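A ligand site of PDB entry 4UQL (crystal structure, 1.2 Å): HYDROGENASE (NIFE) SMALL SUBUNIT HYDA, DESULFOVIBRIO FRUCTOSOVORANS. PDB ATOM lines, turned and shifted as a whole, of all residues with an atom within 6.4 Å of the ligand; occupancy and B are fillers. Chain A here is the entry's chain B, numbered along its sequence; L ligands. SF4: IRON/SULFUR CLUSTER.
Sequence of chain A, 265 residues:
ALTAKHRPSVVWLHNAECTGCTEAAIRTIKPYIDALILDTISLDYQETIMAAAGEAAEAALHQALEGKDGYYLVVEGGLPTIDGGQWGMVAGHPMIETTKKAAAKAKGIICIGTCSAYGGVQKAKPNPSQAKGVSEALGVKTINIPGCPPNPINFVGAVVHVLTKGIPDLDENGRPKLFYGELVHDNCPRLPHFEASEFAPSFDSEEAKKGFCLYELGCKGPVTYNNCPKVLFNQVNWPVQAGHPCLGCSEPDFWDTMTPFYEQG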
ATOM      1  N   VAL A 184      27.639  15.613 -11.499  1.00  0.00           N
ATOM      2  CA  VAL A 184      26.461  15.976 -10.709  1.00  0.00           C
ATOM      3  C   VAL A 184      25.503  16.801 -11.584  1.00  0.00           C
ATOM      4  O   VAL A 184      24.306  16.533 -11.679  1.00  0.00           O
ATOM      5  CB  VAL A 184      26.912  16.720  -9.434  1.00  0.00           C
ATOM      6  CG1 VAL A 184      25.760  17.424  -8.771  1.00  0.00           C
ATOM      7  CG2 VAL A 184      27.579  15.783  -8.481  1.00  0.00           C
ATOM      8  N   HIS A 185      26.065  17.801 -12.228  1.00  0.00           N
ATOM      9  CA  HIS A 185      25.264  18.769 -13.014  1.00  0.00           C
ATOM     10  C   HIS A 185      24.483  18.102 -14.122  1.00  0.00           C
ATOM     11  O   HIS A 185      23.387  18.542 -14.446  1.00  0.00           O
ATOM     12  CB  HIS A 185      26.273  19.742 -13.577  1.00  0.00           C
ATOM     13  CG  HIS A 185      25.739  20.778 -14.536  1.00  0.00           C
ATOM     14  ND1 HIS A 185      25.020  21.878 -14.139  1.00  0.00           N
ATOM     15  CD2 HIS A 185      25.943  20.914 -15.865  1.00  0.00           C
ATOM     16  CE1 HIS A 185      24.802  22.643 -15.205  1.00  0.00           C
ATOM     17  NE2 HIS A 185      25.350  22.078 -16.256  1.00  0.00           N
ATOM     18  N   ASP A 186      25.048  17.072 -14.762  1.00  0.00           N
ATOM     19  CA  ASP A 186      24.382  16.479 -15.904  1.00  0.00           C
ATOM     20  C   ASP A 186      23.083  15.800 -15.540  1.00  0.00           C
ATOM     21  O   ASP A 186      22.233  15.644 -16.400  1.00  0.00           O
ATOM     22  CB  ASP A 186      25.365  15.628 -16.714  1.00  0.00           C
ATOM     23  CG  ASP A 186      26.386  16.489 -17.497  1.00  0.00           C
ATOM     24  OD1 ASP A 186      26.244  17.756 -17.623  1.00  0.00           O
ATOM     25  OD2 ASP A 186      27.317  15.875 -17.994  1.00  0.00           O
ATOM     26  N   CYS A 188      21.243  17.007 -12.725  1.00  0.00           N
ATOM     27  CA  CYS A 188      20.598  17.876 -11.770  1.00  0.00           C
ATOM     28  C   CYS A 188      19.202  18.300 -12.317  1.00  0.00           C
ATOM     29  O   CYS A 188      19.102  18.751 -13.450  1.00  0.00           O
ATOM     30  CB  CYS A 188      21.460  19.141 -11.604  1.00  0.00           C
ATOM     31  SG  CYS A 188      20.680  20.245 -10.394  1.00  0.00           S
ATOM     32  N   PRO A 189      18.141  18.209 -11.515  1.00  0.00           N
ATOM     33  CA  PRO A 189      16.856  18.709 -11.971  1.00  0.00           C
ATOM     34  C   PRO A 189      16.779  20.187 -12.234  1.00  0.00           C
ATOM     35  O   PRO A 189      15.779  20.616 -12.794  1.00  0.00           O
ATOM     36  CB  PRO A 189      15.891  18.321 -10.838  1.00  0.00           C
ATOM     37  CG  PRO A 189      16.530  17.185 -10.164  1.00  0.00           C
ATOM     38  CD  PRO A 189      18.015  17.512 -10.220  1.00  0.00           C
ATOM     39  N   ARG A 190      17.772  20.973 -11.820  1.00  0.00           N
ATOM     40  CA  ARG A 190      17.795  22.402 -12.108  1.00  0.00           C
ATOM     41  C   ARG A 190      18.471  22.696 -13.436  1.00  0.00           C
ATOM     42  O   ARG A 190      18.568  23.875 -13.834  1.00  0.00           O
ATOM     43  CB  ARG A 190      18.421  23.189 -10.961  1.00  0.00           C
ATOM     44  CG  ARG A 190      17.640  22.981  -9.648  1.00  0.00           C
ATOM     45  CD  ARG A 190      18.013  23.941  -8.571  1.00  0.00           C
ATOM     46  NE  ARG A 190      17.273  23.625  -7.356  1.00  0.00           N
ATOM     47  CZ  ARG A 190      17.025  24.454  -6.362  1.00  0.00           C
ATOM     48  NH1 ARG A 190      17.480  25.691  -6.362  1.00  0.00           N
ATOM     49  NH2 ARG A 190      16.358  24.048  -5.313  1.00  0.00           N
ATOM     50  N   LEU A 191      18.949  21.655 -14.123  1.00  0.00           N
ATOM     51  CA  LEU A 191      19.634  21.815 -15.412  1.00  0.00           C
ATOM     52  C   LEU A 191      18.847  22.659 -16.436  1.00  0.00           C
ATOM     53  O   LEU A 191      19.439  23.550 -17.088  1.00  0.00           O
ATOM     54  CB  LEU A 191      20.093  20.487 -15.974  1.00  0.00           C
ATOM     55  CG  LEU A 191      20.955  20.563 -17.233  1.00  0.00           C
ATOM     56  CD1 LEU A 191      22.262  21.274 -17.000  1.00  0.00           C
ATOM     57  CD2 LEU A 191      21.239  19.171 -17.751  1.00  0.00           C
ATOM     58  N   PRO A 192      17.495  22.480 -16.556  1.00  0.00           N
ATOM     59  CA  PRO A 192      16.785  23.342 -17.512  1.00  0.00           C
ATOM     60  C   PRO A 192      16.888  24.826 -17.142  1.00  0.00           C
ATOM     61  O   PRO A 192      16.911  25.667 -18.011  1.00  0.00           O
ATOM     62  CB  PRO A 192      15.330  22.803 -17.441  1.00  0.00           C
ATOM     63  CG  PRO A 192      15.490  21.420 -16.978  1.00  0.00           C
ATOM     64  CD  PRO A 192      16.647  21.398 -16.029  1.00  0.00           C
ATOM     65  N   HIS A 193      16.944  25.140 -15.833  1.00  0.00           N
ATOM     66  CA  HIS A 193      17.188  26.558 -15.443  1.00  0.00           C
ATOM     67  C   HIS A 193      18.579  26.988 -15.853  1.00  0.00           C
ATOM     68  O   HIS A 193      18.752  28.113 -16.377  1.00  0.00           O
ATOM     69  CB  HIS A 193      16.995  26.801 -13.947  1.00  0.00           C
ATOM     70  CG  HIS A 193      15.561  26.705 -13.498  1.00  0.00           C
ATOM     71  ND1 HIS A 193      14.546  27.411 -14.110  1.00  0.00           N
ATOM     72  CD2 HIS A 193      14.978  25.979 -12.525  1.00  0.00           C
ATOM     73  CE1 HIS A 193      13.390  27.164 -13.496  1.00  0.00           C
ATOM     74  NE2 HIS A 193      13.626  26.278 -12.559  1.00  0.00           N
ATOM     75  N   PHE A 194      19.584  26.165 -15.562  1.00  0.00           N
ATOM     76  CA  PHE A 194      20.949  26.504 -15.980  1.00  0.00           C
ATOM     77  C   PHE A 194      20.997  26.840 -17.486  1.00  0.00           C
ATOM     78  O   PHE A 194      21.557  27.847 -17.895  1.00  0.00           O
ATOM     79  CB  PHE A 194      21.931  25.382 -15.604  1.00  0.00           C
ATOM     80  CG  PHE A 194      23.340  25.592 -16.106  1.00  0.00           C
ATOM     81  CD1 PHE A 194      24.284  26.271 -15.330  1.00  0.00           C
ATOM     82  CD2 PHE A 194      23.750  25.084 -17.316  1.00  0.00           C
ATOM     83  CE1 PHE A 194      25.548  26.480 -15.772  1.00  0.00           C
ATOM     84  CE2 PHE A 194      25.075  25.222 -17.751  1.00  0.00           C
ATOM     85  CZ  PHE A 194      25.974  25.928 -16.963  1.00  0.00           C
ATOM     86  N   PHE A 199      19.074  31.865 -12.784  1.00  0.00           N
ATOM     87  CA  PHE A 199      19.929  31.696 -11.597  1.00  0.00           C
ATOM     88  C   PHE A 199      19.339  32.452 -10.421  1.00  0.00           C
ATOM     89  O   PHE A 199      18.818  33.538 -10.544  1.00  0.00           O
ATOM     90  CB  PHE A 199      21.326  32.268 -11.880  1.00  0.00           C
ATOM     91  CG  PHE A 199      21.989  31.675 -13.075  1.00  0.00           C
ATOM     92  CD1 PHE A 199      22.427  30.382 -13.061  1.00  0.00           C
ATOM     93  CD2 PHE A 199      22.289  32.425 -14.212  1.00  0.00           C
ATOM     94  CE1 PHE A 199      23.049  29.782 -14.116  1.00  0.00           C
ATOM     95  CE2 PHE A 199      22.926  31.842 -15.267  1.00  0.00           C
ATOM     96  CZ  PHE A 199      23.315  30.519 -15.230  1.00  0.00           C
ATOM     97  N   PHE A 212      15.522  28.121  -8.905  1.00  0.00           N
ATOM     98  CA  PHE A 212      16.468  28.435  -9.991  1.00  0.00           C
ATOM     99  C   PHE A 212      17.853  27.833  -9.708  1.00  0.00           C
ATOM    100  O   PHE A 212      18.132  27.433  -8.579  1.00  0.00           O
ATOM    101  CB  PHE A 212      16.558  29.943 -10.213  1.00  0.00           C
ATOM    102  CG  PHE A 212      15.407  30.552 -11.012  1.00  0.00           C
ATOM    103  CD1 PHE A 212      14.190  29.925 -11.176  1.00  0.00           C
ATOM    104  CD2 PHE A 212      15.594  31.805 -11.590  1.00  0.00           C
ATOM    105  CE1 PHE A 212      13.177  30.522 -11.903  1.00  0.00           C
ATOM    106  CE2 PHE A 212      14.566  32.410 -12.318  1.00  0.00           C
ATOM    107  CZ  PHE A 212      13.377  31.775 -12.475  1.00  0.00           C
ATOM    108  N   CYS A 213      18.679  27.767 -10.751  1.00  0.00           N
ATOM    109  CA  CYS A 213      19.980  27.164 -10.622  1.00  0.00           C
ATOM    110  C   CYS A 213      20.862  27.942  -9.668  1.00  0.00           C
ATOM    111  O   CYS A 213      20.754  29.171  -9.549  1.00  0.00           O
ATOM    112  CB  CYS A 213      20.590  27.110 -12.002  1.00  0.00           C
ATOM    113  SG  CYS A 213      22.352  26.716 -12.086  1.00  0.00           S
ATOM    114  N   LEU A 214      21.694  27.200  -8.945  1.00  0.00           N
ATOM    115  CA  LEU A 214      22.561  27.751  -7.863  1.00  0.00           C
ATOM    116  C   LEU A 214      24.005  28.052  -8.315  1.00  0.00           C
ATOM    117  O   LEU A 214      24.890  28.275  -7.500  1.00  0.00           O
ATOM    118  CB  LEU A 214      22.562  26.733  -6.752  1.00  0.00           C
ATOM    119  CG  LEU A 214      21.192  26.413  -6.176  1.00  0.00           C
ATOM    120  CD1 LEU A 214      21.318  25.331  -5.110  1.00  0.00           C
ATOM    121  CD2 LEU A 214      20.501  27.627  -5.579  1.00  0.00           C
ATOM    122  N   TYR A 215      24.243  28.111  -9.625  1.00  0.00           N
ATOM    123  CA  TYR A 215      25.585  28.328 -10.152  1.00  0.00           C
ATOM    124  C   TYR A 215      26.217  29.652  -9.684  1.00  0.00           C
ATOM    125  O   TYR A 215      27.403  29.697  -9.351  1.00  0.00           O
ATOM    126  CB  TYR A 215      25.600  28.218 -11.677  1.00  0.00           C
ATOM    127  CG  TYR A 215      26.977  28.162 -12.245  1.00  0.00           C
ATOM    128  CD1 TYR A 215      27.729  27.002 -12.176  1.00  0.00           C
ATOM    129  CD2 TYR A 215      27.568  29.281 -12.810  1.00  0.00           C
ATOM    130  CE1 TYR A 215      29.023  26.939 -12.681  1.00  0.00           C
ATOM    131  CE2 TYR A 215      28.848  29.229 -13.302  1.00  0.00           C
ATOM    132  CZ  TYR A 215      29.559  28.052 -13.246  1.00  0.00           C
ATOM    133  OH  TYR A 215      30.861  27.944 -13.717  1.00  0.00           O
ATOM    134  N   CYS A 219      27.779  26.844  -7.056  1.00  0.00           N
ATOM    135  CA  CYS A 219      27.589  25.410  -7.261  1.00  0.00           C
ATOM    136  C   CYS A 219      28.704  24.800  -8.067  1.00  0.00           C
ATOM    137  O   CYS A 219      28.986  25.268  -9.199  1.00  0.00           O
ATOM    138  CB  CYS A 219      26.271  25.139  -7.980  1.00  0.00           C
ATOM    139  SG  CYS A 219      25.846  23.396  -7.914  1.00  0.00           S
ATOM    140  N   LYS A 220      29.333  23.762  -7.510  1.00  0.00           N
ATOM    141  CA  LYS A 220      30.384  23.007  -8.222  1.00  0.00           C
ATOM    142  C   LYS A 220      29.883  21.770  -8.907  1.00  0.00           C
ATOM    143  O   LYS A 220      30.670  21.004  -9.455  1.00  0.00           O
ATOM    144  CB  LYS A 220      31.518  22.677  -7.253  1.00  0.00           C
ATOM    145  CG  LYS A 220      32.071  23.915  -6.544  1.00  0.00           C
ATOM    146  CD  LYS A 220      32.539  24.984  -7.511  1.00  0.00           C
ATOM    147  CE  LYS A 220      33.304  26.149  -6.883  1.00  0.00           C
ATOM    148  NZ  LYS A 220      32.615  26.741  -5.700  1.00  0.00           N
ATOM    149  N   GLY A 221      28.568  21.600  -9.042  1.00  0.00           N
ATOM    150  CA  GLY A 221      28.034  20.461  -9.797  1.00  0.00           C
ATOM    151  C   GLY A 221      28.631  20.317 -11.178  1.00  0.00           C
ATOM    152  O   GLY A 221      28.882  19.193 -11.610  1.00  0.00           O
ATOM    153  N   PRO A 222      28.852  21.429 -11.903  1.00  0.00           N
ATOM    154  CA  PRO A 222      29.439  21.308 -13.231  1.00  0.00           C
ATOM    155  C   PRO A 222      30.828  20.742 -13.360  1.00  0.00           C
ATOM    156  O   PRO A 222      31.233  20.438 -14.504  1.00  0.00           O
ATOM    157  CB  PRO A 222      29.333  22.738 -13.796  1.00  0.00           C
ATOM    158  CG  PRO A 222      28.204  23.381 -13.027  1.00  0.00           C
ATOM    159  CD  PRO A 222      28.361  22.807 -11.641  1.00  0.00           C
ATOM    160  N   TRP A 238      19.005  15.675  -1.632  1.00  0.00           N
ATOM    161  CA  TRP A 238      20.432  15.933  -1.876  1.00  0.00           C
ATOM    162  C   TRP A 238      20.646  17.447  -1.779  1.00  0.00           C
ATOM    163  O   TRP A 238      19.671  18.190  -1.746  1.00  0.00           O
ATOM    164  CB  TRP A 238      20.911  15.347  -3.196  1.00  0.00           C
ATOM    165  CG  TRP A 238      20.409  16.027  -4.467  1.00  0.00           C
ATOM    166  CD1 TRP A 238      19.128  16.049  -4.952  1.00  0.00           C
ATOM    167  CD2 TRP A 238      21.223  16.768  -5.401  1.00  0.00           C
ATOM    168  NE1 TRP A 238      19.104  16.752  -6.145  1.00  0.00           N
ATOM    169  CE2 TRP A 238      20.368  17.197  -6.436  1.00  0.00           C
ATOM    170  CE3 TRP A 238      22.574  17.083  -5.469  1.00  0.00           C
ATOM    171  CZ2 TRP A 238      20.868  17.941  -7.516  1.00  0.00           C
ATOM    172  CZ3 TRP A 238      23.055  17.818  -6.508  1.00  0.00           C
ATOM    173  CH2 TRP A 238      22.208  18.252  -7.545  1.00  0.00           C
ATOM    174  N   VAL A 240      21.369  20.185  -3.544  1.00  0.00           N
ATOM    175  CA  VAL A 240      20.747  21.180  -4.430  1.00  0.00           C
ATOM    176  C   VAL A 240      19.222  21.136  -4.239  1.00  0.00           C
ATOM    177  O   VAL A 240      18.555  22.185  -4.284  1.00  0.00           O
ATOM    178  CB  VAL A 240      21.176  20.961  -5.898  1.00  0.00           C
ATOM    179  CG1 VAL A 240      20.257  21.702  -6.834  1.00  0.00           C
ATOM    180  CG2 VAL A 240      22.635  21.330  -6.067  1.00  0.00           C
ATOM    181  N   PRO A 245      24.247  25.015  -2.956  1.00  0.00           N
ATOM    182  CA  PRO A 245      25.181  24.539  -3.984  1.00  0.00           C
ATOM    183  C   PRO A 245      25.993  23.338  -3.575  1.00  0.00           C
ATOM    184  O   PRO A 245      26.219  23.107  -2.409  1.00  0.00           O
ATOM    185  CB  PRO A 245      26.101  25.760  -4.175  1.00  0.00           C
ATOM    186  CG  PRO A 245      25.953  26.607  -2.930  1.00  0.00           C
ATOM    187  CD  PRO A 245      24.491  26.417  -2.598  1.00  0.00           C
ATOM    188  N   CYS A 246      26.398  22.538  -4.571  1.00  0.00           N
ATOM    189  CA  CYS A 246      27.397  21.496  -4.421  1.00  0.00           C
ATOM    190  C   CYS A 246      28.743  22.122  -4.114  1.00  0.00           C
ATOM    191  O   CYS A 246      29.119  23.157  -4.698  1.00  0.00           O
ATOM    192  CB  CYS A 246      27.407  20.690  -5.724  1.00  0.00           C
ATOM    193  SG  CYS A 246      28.707  19.407  -5.866  1.00  0.00           S
ATOM    194  N   GLN A 264      32.510  31.298  -7.930  1.00  0.00           N
ATOM    195  CA  GLN A 264      33.148  30.519  -9.008  1.00  0.00           C
ATOM    196  C   GLN A 264      34.623  30.937  -9.149  1.00  0.00           C
ATOM    197  O   GLN A 264      34.918  31.758  -9.980  1.00  0.00           O
ATOM    198  CB  GLN A 264      32.346  30.654 -10.324  1.00  0.00           C
ATOM    199  CG  GLN A 264      30.921  30.083 -10.246  1.00  0.00           C
ATOM    200  CD  GLN A 264      30.909  28.578 -10.026  1.00  0.00           C
ATOM    201  OE1 GLN A 264      31.910  27.869 -10.250  1.00  0.00           O
ATOM    202  NE2 GLN A 264      29.758  28.058  -9.620  1.00  0.00           N
HETATM  203 FE1  SF4 L   1      22.706  24.553 -11.454  1.00  0.00          FE
HETATM  204 FE2  SF4 L   1      22.148  21.992 -10.686  1.00  0.00          FE
HETATM  205 FE3  SF4 L   1      24.230  22.499 -12.294  1.00  0.00          FE
HETATM  206 FE4  SF4 L   1      24.362  23.230  -9.671  1.00  0.00          FE
HETATM  207  S1  SF4 L   1      24.294  21.082 -10.506  1.00  0.00           S
HETATM  208  S2  SF4 L   1      25.025  24.472 -11.480  1.00  0.00           S
HETATM  209  S3  SF4 L   1      22.140  23.836  -9.352  1.00  0.00           S
HETATM  210  S4  SF4 L   1      22.006  22.854 -12.804  1.00  0.00           S
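ND1 of His 185 binds FE3 of the ligand (2.1 Å). The side-chain sulfur (SG) of Cys 213 binds an iron atom (FE1) of the ligand, at 2.3 Å. SG of Cys 188 is bound to FE2 of the ligand (2.3 Å). The side-chain sulfur (SG) of Cys 219 is bound to an iron atom (FE4) of the ligand (2.3 Å). N of Leu 214 lies close to S3 of the ligand. S4 of the ligand sits close to N of Leu 191 (3.5 Å).
The backbone NH (N) of Arg 190 lies close to the side-chain sulfur (SG) of Cys 188 (3.3 Å). N of Cys 219 lies within hydrogen-bond range of O of Leu 214. N of Gly 221 lies close to SG of Cys 219 (3.5 Å). The side-chain sulfur (SG) of Cys 219 sits close to the backbone NH (N) of Cys 246 (3.5 Å). The backbone carbonyl oxygen (O) of Cys 219 is in hydrogen-bond range of the side-chain amide nitrogen (NE2) of Gln 264. O of Val 240 is in hydrogen-bond range of NH2 of Arg 190, at 3.1 Å. The guanidinium group (NH1) of Arg 190 lies within hydrogen-bond range of the backbone carbonyl oxygen (O) of Phe 212, 2.9 Å away. The backbone carbonyl oxygen of Tyr 215 sits at hydrogen-bond distance from the side-chain amide nitrogen of Gln 264 (2.9 Å).
A sulfur (S4) of the ligand lies close to the backbone carbonyl oxygen of Arg 190, 3.7 Å away. Phe 194 touches the ligand. Tyr 215 touches the ligand (CD1 to S2, 3.8 Å). Gly 221 touches the ligand (CA to S1, 3.9 Å). CG of Pro 222 touches S2 of the ligand (3.7 Å). Val 240 touches the ligand. Hydrophobic or aromatic side chains within 4 Å of the ligand: His 185, Phe 194, Leu 214, Tyr 215, Pro 222 and Val 240. Within 4 Å of the ligand: His 185, Cys 188, Arg 190, Leu 191, Phe 194, Cys 213, Leu 214, Tyr 215, Cys 219, Gly 221, Pro 222 and Val 240. The nearest printed residue that does not touch the ligand is Val 184 (4.3 Å).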
